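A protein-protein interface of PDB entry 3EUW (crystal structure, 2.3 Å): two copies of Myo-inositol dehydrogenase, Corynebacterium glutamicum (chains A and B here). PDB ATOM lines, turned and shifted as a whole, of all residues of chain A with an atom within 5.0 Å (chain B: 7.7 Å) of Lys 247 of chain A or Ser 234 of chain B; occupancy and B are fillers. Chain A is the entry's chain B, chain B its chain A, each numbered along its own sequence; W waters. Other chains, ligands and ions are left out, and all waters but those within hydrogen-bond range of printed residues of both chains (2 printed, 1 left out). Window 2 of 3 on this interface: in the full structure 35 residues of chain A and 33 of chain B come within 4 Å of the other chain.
The backbone NH (N) of Gly 248 of chain A lies close to the side-chain hydroxyl (OG) of Ser 234 of chain B (3.2 Å).
The backbone NH of Ser 246 of chain A lies within hydrogen-bond range of the backbone carbonyl oxygen of Ile 143 of chain A, at 3.3 Å. The backbone carbonyl oxygen (O) of Asp 155 of chain B lies close to the backbone NH (N) of His 232 of chain B, at 3.2 Å. The side-chain sulfur (SG) of Cys 233 of chain B sits close to the side-chain hydroxyl (OH) of Tyr 235 of chain B, 3.7 Å away. The backbone carbonyl oxygen (O) of Ile 143 of chain A lies within hydrogen-bond range of the backbone NH (N) of Lys 247 of chain A, at 2.8 Å. The backbone carbonyl oxygen of Tyr 235 of chain B sits at hydrogen-bond distance from the backbone NH of Ile 274 of chain B, at 3.0 Å. NH1 of Arg 154 of chain B lies within hydrogen-bond range of OH of Tyr 235 of chain B (3.3 Å).
Among the printed residues, merely in contact across the chains: Ser 246 of chain A with His 232 of chain B (3.9 Å), Lys 247 of chain A with Ser 234 of chain B (3.5 Å) and Met 249 of chain A with Tyr 235 of chain B (3.8 Å).
Of chain B, only Ser 234 (3.5 Å) comes within 4 Å of Lys 247 of chain A. Of chain A, only Lys 247 (3.5 Å) and Gly 248 (3.2 Å) come within 4 Å of Ser 234 of chain B. Ser 246 of chain A touches just one residue of chain B: His 232. Of the printed residues of chain A, His 232 of chain B touches Ser 246 (3.9 Å). Of the printed residues of chain A, Tyr 235 of chain B touches Met 249 (3.8 Å). The nearest residue of chain B that does not touch Lys 247 of chain A is His 232 of chain B (6.0 Å). The nearest printed residue of chain A that does not touch Tyr 235 of chain B is Gly 248 of chain A (4.8 Å).
Printed residues of chain B that touch a printed residue of chain A: His 232, Ser 234 and Tyr 235. Hydrophobic or aromatic side chains of chain A within 4 Å of the printed part of chain B: Met 249. Among the printed residues, 4 pairs touch across the chains. Among the printed residues, no Asp or Glu carboxylate lies within 4 Å of a Lys or Arg side-chain nitrogen of the other chain.
No position is printed for both chains.
Water W2 lies within hydrogen-bond range of the backbone carbonyl oxygen of Ser 246 of chain A (2.7 Å) and a ring nitrogen (ND1) of His 232 of chain B (3.2 Å). Water W1 lies within hydrogen-bond range of the backbone NH of Ser 234 of chain B, the backbone carbonyl oxygen of Gly 245 of chain A and the backbone carbonyl oxygen of Ser 246 of chain A.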
ATOM      1  N   GLU A 142      10.684  -7.697  -9.828  1.00  0.00           N
ATOM      2  CA  GLU A 142      10.651  -7.540  -8.374  1.00  0.00           C
ATOM      3  C   GLU A 142      11.651  -8.391  -7.582  1.00  0.00           C
ATOM      4  O   GLU A 142      12.027  -8.026  -6.468  1.00  0.00           O
ATOM      5  CB  GLU A 142       9.235  -7.783  -7.836  1.00  0.00           C
ATOM      6  CG  GLU A 142       8.977  -7.023  -6.539  1.00  0.00           C
ATOM      7  CD  GLU A 142       7.573  -7.182  -5.994  1.00  0.00           C
ATOM      8  OE1 GLU A 142       6.613  -7.226  -6.791  1.00  0.00           O
ATOM      9  OE2 GLU A 142       7.426  -7.242  -4.755  1.00  0.00           O
ATOM     10  N   ILE A 143      12.077  -9.519  -8.139  1.00  0.00           N
ATOM     11  CA  ILE A 143      13.038 -10.350  -7.430  1.00  0.00           C
ATOM     12  C   ILE A 143      14.281 -10.633  -8.263  1.00  0.00           C
ATOM     13  O   ILE A 143      14.981 -11.616  -8.023  1.00  0.00           O
ATOM     14  CB  ILE A 143      12.426 -11.688  -6.981  1.00  0.00           C
ATOM     15  CG1 ILE A 143      11.925 -12.481  -8.188  1.00  0.00           C
ATOM     16  CG2 ILE A 143      11.304 -11.430  -5.994  1.00  0.00           C
ATOM     17  CD1 ILE A 143      11.494 -13.899  -7.828  1.00  0.00           C
ATOM     18  N   GLY A 144      14.546  -9.761  -9.234  1.00  0.00           N
ATOM     19  CA  GLY A 144      15.715  -9.913 -10.087  1.00  0.00           C
ATOM     20  C   GLY A 144      15.540 -11.002 -11.122  1.00  0.00           C
ATOM     21  O   GLY A 144      14.417 -11.360 -11.448  1.00  0.00           O
ATOM     22  N   GLY A 245      14.751 -15.747  -7.154  1.00  0.00           N
ATOM     23  CA  GLY A 245      15.555 -14.917  -8.031  1.00  0.00           C
ATOM     24  C   GLY A 245      16.783 -14.324  -7.367  1.00  0.00           C
ATOM     25  O   GLY A 245      16.977 -14.448  -6.152  1.00  0.00           O
ATOM     26  N   SER A 246      17.608 -13.673  -8.177  1.00  0.00           N
ATOM     27  CA  SER A 246      18.840 -13.049  -7.716  1.00  0.00           C
ATOM     28  C   SER A 246      18.628 -11.953  -6.668  1.00  0.00           C
ATOM     29  O   SER A 246      19.546 -11.641  -5.922  1.00  0.00           O
ATOM     30  CB  SER A 246      19.616 -12.473  -8.917  1.00  0.00           C
ATOM     31  OG  SER A 246      18.838 -11.530  -9.635  1.00  0.00           O
ATOM     32  N   LYS A 247      17.430 -11.378  -6.596  1.00  0.00           N
ATOM     33  CA  LYS A 247      17.167 -10.308  -5.628  1.00  0.00           C
ATOM     34  C   LYS A 247      16.090 -10.617  -4.603  1.00  0.00           C
ATOM     35  O   LYS A 247      15.628  -9.718  -3.899  1.00  0.00           O
ATOM     36  CB  LYS A 247      16.782  -9.012  -6.348  1.00  0.00           C
ATOM     37  CG  LYS A 247      17.921  -8.308  -7.072  1.00  0.00           C
ATOM     38  CD  LYS A 247      17.410  -7.069  -7.812  1.00  0.00           C
ATOM     39  CE  LYS A 247      18.523  -6.379  -8.589  1.00  0.00           C
ATOM     40  NZ  LYS A 247      17.998  -5.304  -9.472  1.00  0.00           N
ATOM     41  N   GLY A 248      15.679 -11.875  -4.515  1.00  0.00           N
ATOM     42  CA  GLY A 248      14.653 -12.222  -3.554  1.00  0.00           C
ATOM     43  C   GLY A 248      13.847 -13.437  -3.958  1.00  0.00           C
ATOM     44  O   GLY A 248      14.179 -14.120  -4.932  1.00  0.00           O
ATOM     45  N   MET A 249      12.777 -13.698  -3.217  1.00  0.00           N
ATOM     46  CA  MET A 249      11.935 -14.837  -3.506  1.00  0.00           C
ATOM     47  C   MET A 249      10.451 -14.567  -3.265  1.00  0.00           C
ATOM     48  O   MET A 249      10.085 -13.806  -2.365  1.00  0.00           O
ATOM     49  CB  MET A 249      12.403 -16.025  -2.668  1.00  0.00           C
ATOM     50  CG  MET A 249      11.807 -17.314  -3.117  1.00  0.00           C
ATOM     51  SD  MET A 249      10.398 -17.731  -1.920  1.00  0.00           S
ATOM     52  CE  MET A 249      11.158 -19.331  -1.147  1.00  0.00           C
ATOM     53  N   ARG B 154      20.431 -22.728   0.578  1.00  0.00           N
ATOM     54  CA  ARG B 154      20.999 -21.680  -0.249  1.00  0.00           C
ATOM     55  C   ARG B 154      21.946 -20.838   0.591  1.00  0.00           C
ATOM     56  O   ARG B 154      21.555 -20.275   1.615  1.00  0.00           O
ATOM     57  CB  ARG B 154      19.891 -20.805  -0.842  1.00  0.00           C
ATOM     58  CG  ARG B 154      18.924 -21.570  -1.733  1.00  0.00           C
ATOM     59  CD  ARG B 154      17.756 -20.671  -2.161  1.00  0.00           C
ATOM     60  NE  ARG B 154      16.937 -21.269  -3.207  1.00  0.00           N
ATOM     61  CZ  ARG B 154      15.608 -21.281  -3.210  1.00  0.00           C
ATOM     62  NH1 ARG B 154      14.921 -20.718  -2.214  1.00  0.00           N
ATOM     63  NH2 ARG B 154      14.968 -21.873  -4.201  1.00  0.00           N
ATOM     64  N   ASP B 155      23.204 -20.777   0.173  1.00  0.00           N
ATOM     65  CA  ASP B 155      24.171 -19.980   0.898  1.00  0.00           C
ATOM     66  C   ASP B 155      23.899 -18.513   0.596  1.00  0.00           C
ATOM     67  O   ASP B 155      23.406 -18.175  -0.484  1.00  0.00           O
ATOM     68  CB  ASP B 155      25.598 -20.319   0.468  1.00  0.00           C
ATOM     69  CG  ASP B 155      26.070 -21.642   1.003  1.00  0.00           C
ATOM     70  OD1 ASP B 155      25.315 -22.302   1.751  1.00  0.00           O
ATOM     71  OD2 ASP B 155      27.215 -22.018   0.674  1.00  0.00           O
ATOM     72  N   PRO B 156      24.206 -17.628   1.553  1.00  0.00           N
ATOM     73  CA  PRO B 156      24.008 -16.187   1.395  1.00  0.00           C
ATOM     74  C   PRO B 156      24.780 -15.684   0.184  1.00  0.00           C
ATOM     75  O   PRO B 156      24.255 -14.910  -0.613  1.00  0.00           O
ATOM     76  CB  PRO B 156      24.564 -15.614   2.701  1.00  0.00           C
ATOM     77  CG  PRO B 156      24.244 -16.690   3.687  1.00  0.00           C
ATOM     78  CD  PRO B 156      24.609 -17.957   2.932  1.00  0.00           C
ATOM     79  N   ALA B 157      26.029 -16.130   0.049  1.00  0.00           N
ATOM     80  CA  ALA B 157      26.882 -15.716  -1.076  1.00  0.00           C
ATOM     81  C   ALA B 157      28.033 -16.690  -1.311  1.00  0.00           C
ATOM     82  O   ALA B 157      28.320 -17.536  -0.470  1.00  0.00           O
ATOM     83  CB  ALA B 157      27.452 -14.305  -0.820  1.00  0.00           C
ATOM     84  N   HIS B 232      23.824 -18.304  -3.615  1.00  0.00           N
ATOM     85  CA  HIS B 232      23.524 -16.984  -3.060  1.00  0.00           C
ATOM     86  C   HIS B 232      22.069 -16.929  -2.605  1.00  0.00           C
ATOM     87  O   HIS B 232      21.246 -17.740  -3.036  1.00  0.00           O
ATOM     88  CB  HIS B 232      23.863 -15.824  -4.018  1.00  0.00           C
ATOM     89  CG  HIS B 232      22.987 -15.723  -5.227  1.00  0.00           C
ATOM     90  ND1 HIS B 232      23.147 -14.732  -6.168  1.00  0.00           N
ATOM     91  CD2 HIS B 232      21.937 -16.474  -5.640  1.00  0.00           C
ATOM     92  CE1 HIS B 232      22.229 -14.870  -7.112  1.00  0.00           C
ATOM     93  NE2 HIS B 232      21.484 -15.918  -6.814  1.00  0.00           N
ATOM     94  N   CYS B 233      21.760 -15.992  -1.715  1.00  0.00           N
ATOM     95  CA  CYS B 233      20.412 -15.872  -1.176  1.00  0.00           C
ATOM     96  C   CYS B 233      20.299 -14.517  -0.498  1.00  0.00           C
ATOM     97  O   CYS B 233      20.944 -14.266   0.514  1.00  0.00           O
ATOM     98  CB  CYS B 233      20.161 -16.990  -0.166  1.00  0.00           C
ATOM     99  SG  CYS B 233      18.508 -17.013   0.560  1.00  0.00           S
ATOM    100  N   SER B 234      19.456 -13.657  -1.052  1.00  0.00           N
ATOM    101  CA  SER B 234      19.310 -12.297  -0.554  1.00  0.00           C
ATOM    102  C   SER B 234      18.785 -12.125   0.866  1.00  0.00           C
ATOM    103  O   SER B 234      19.133 -11.156   1.531  1.00  0.00           O
ATOM    104  CB  SER B 234      18.444 -11.481  -1.522  1.00  0.00           C
ATOM    105  OG  SER B 234      17.133 -12.003  -1.615  1.00  0.00           O
ATOM    106  N   TYR B 235      17.983 -13.069   1.346  1.00  0.00           N
ATOM    107  CA  TYR B 235      17.410 -12.940   2.680  1.00  0.00           C
ATOM    108  C   TYR B 235      18.108 -13.699   3.808  1.00  0.00           C
ATOM    109  O   TYR B 235      17.612 -13.722   4.930  1.00  0.00           O
ATOM    110  CB  TYR B 235      15.933 -13.325   2.628  1.00  0.00           C
ATOM    111  CG  TYR B 235      15.677 -14.651   1.937  1.00  0.00           C
ATOM    112  CD1 TYR B 235      15.798 -15.862   2.631  1.00  0.00           C
ATOM    113  CD2 TYR B 235      15.334 -14.695   0.585  1.00  0.00           C
ATOM    114  CE1 TYR B 235      15.584 -17.091   1.989  1.00  0.00           C
ATOM    115  CE2 TYR B 235      15.112 -15.911  -0.071  1.00  0.00           C
ATOM    116  CZ  TYR B 235      15.242 -17.104   0.635  1.00  0.00           C
ATOM    117  OH  TYR B 235      15.040 -18.289  -0.028  1.00  0.00           O
ATOM    118  N   GLY B 236      19.256 -14.306   3.516  1.00  0.00           N
ATOM    119  CA  GLY B 236      19.974 -15.032   4.548  1.00  0.00           C
ATOM    120  C   GLY B 236      20.398 -16.435   4.166  1.00  0.00           C
ATOM    121  O   GLY B 236      20.511 -16.762   2.988  1.00  0.00           O
ATOM    122  N   TYR B 237      20.623 -17.266   5.183  1.00  0.00           N
ATOM    123  CA  TYR B 237      21.065 -18.649   5.018  1.00  0.00           C
ATOM    124  C   TYR B 237      19.850 -19.592   5.027  1.00  0.00           C
ATOM    125  O   TYR B 237      19.430 -20.078   6.075  1.00  0.00           O
ATOM    126  CB  TYR B 237      22.034 -18.977   6.159  1.00  0.00           C
ATOM    127  CG  TYR B 237      22.741 -20.313   6.087  1.00  0.00           C
ATOM    128  CD1 TYR B 237      23.106 -20.875   4.863  1.00  0.00           C
ATOM    129  CD2 TYR B 237      23.125 -20.974   7.254  1.00  0.00           C
ATOM    130  CE1 TYR B 237      23.843 -22.057   4.802  1.00  0.00           C
ATOM    131  CE2 TYR B 237      23.862 -22.159   7.205  1.00  0.00           C
ATOM    132  CZ  TYR B 237      24.218 -22.691   5.978  1.00  0.00           C
ATOM    133  OH  TYR B 237      24.953 -23.846   5.928  1.00  0.00           O
ATOM    134  N   PRO B 273      15.229 -10.671   8.333  1.00  0.00           N
ATOM    135  CA  PRO B 273      15.833 -11.532   7.322  1.00  0.00           C
ATOM    136  C   PRO B 273      16.287 -12.694   8.219  1.00  0.00           C
ATOM    137  O   PRO B 273      16.506 -12.496   9.421  1.00  0.00           O
ATOM    138  CB  PRO B 273      17.018 -10.700   6.828  1.00  0.00           C
ATOM    139  CG  PRO B 273      16.515  -9.296   6.959  1.00  0.00           C
ATOM    140  CD  PRO B 273      15.825  -9.325   8.307  1.00  0.00           C
ATOM    141  N   ILE B 274      16.425 -13.890   7.674  1.00  0.00           N
ATOM    142  CA  ILE B 274      16.827 -15.007   8.516  1.00  0.00           C
ATOM    143  C   ILE B 274      18.326 -14.969   8.800  1.00  0.00           C
ATOM    144  O   ILE B 274      19.049 -14.196   8.179  1.00  0.00           O
ATOM    145  CB  ILE B 274      16.447 -16.329   7.858  1.00  0.00           C
ATOM    146  CG1 ILE B 274      17.261 -16.538   6.572  1.00  0.00           C
ATOM    147  CG2 ILE B 274      14.951 -16.309   7.552  1.00  0.00           C
ATOM    148  CD1 ILE B 274      17.001 -17.895   5.884  1.00  0.00           C
ATOM    149  N   ASN B 276      22.135 -15.108   8.747  1.00  0.00           N
ATOM    150  CA  ASN B 276      23.024 -15.046   7.603  1.00  0.00           C
ATOM    151  C   ASN B 276      24.267 -15.921   7.711  1.00  0.00           C
ATOM    152  O   ASN B 276      24.851 -16.290   6.700  1.00  0.00           O
ATOM    153  CB  ASN B 276      23.473 -13.599   7.385  1.00  0.00           C
ATOM    154  CG  ASN B 276      24.196 -13.413   6.070  1.00  0.00           C
ATOM    155  OD1 ASN B 276      23.563 -13.274   5.021  1.00  0.00           O
ATOM    156  ND2 ASN B 276      25.527 -13.431   6.112  1.00  0.00           N
HETATM  157  O   HOH W   1      18.627 -14.006  -3.653  1.00  0.00           O
HETATM  158  O   HOH W   2      20.978 -13.285  -4.290  1.00  0.00           O
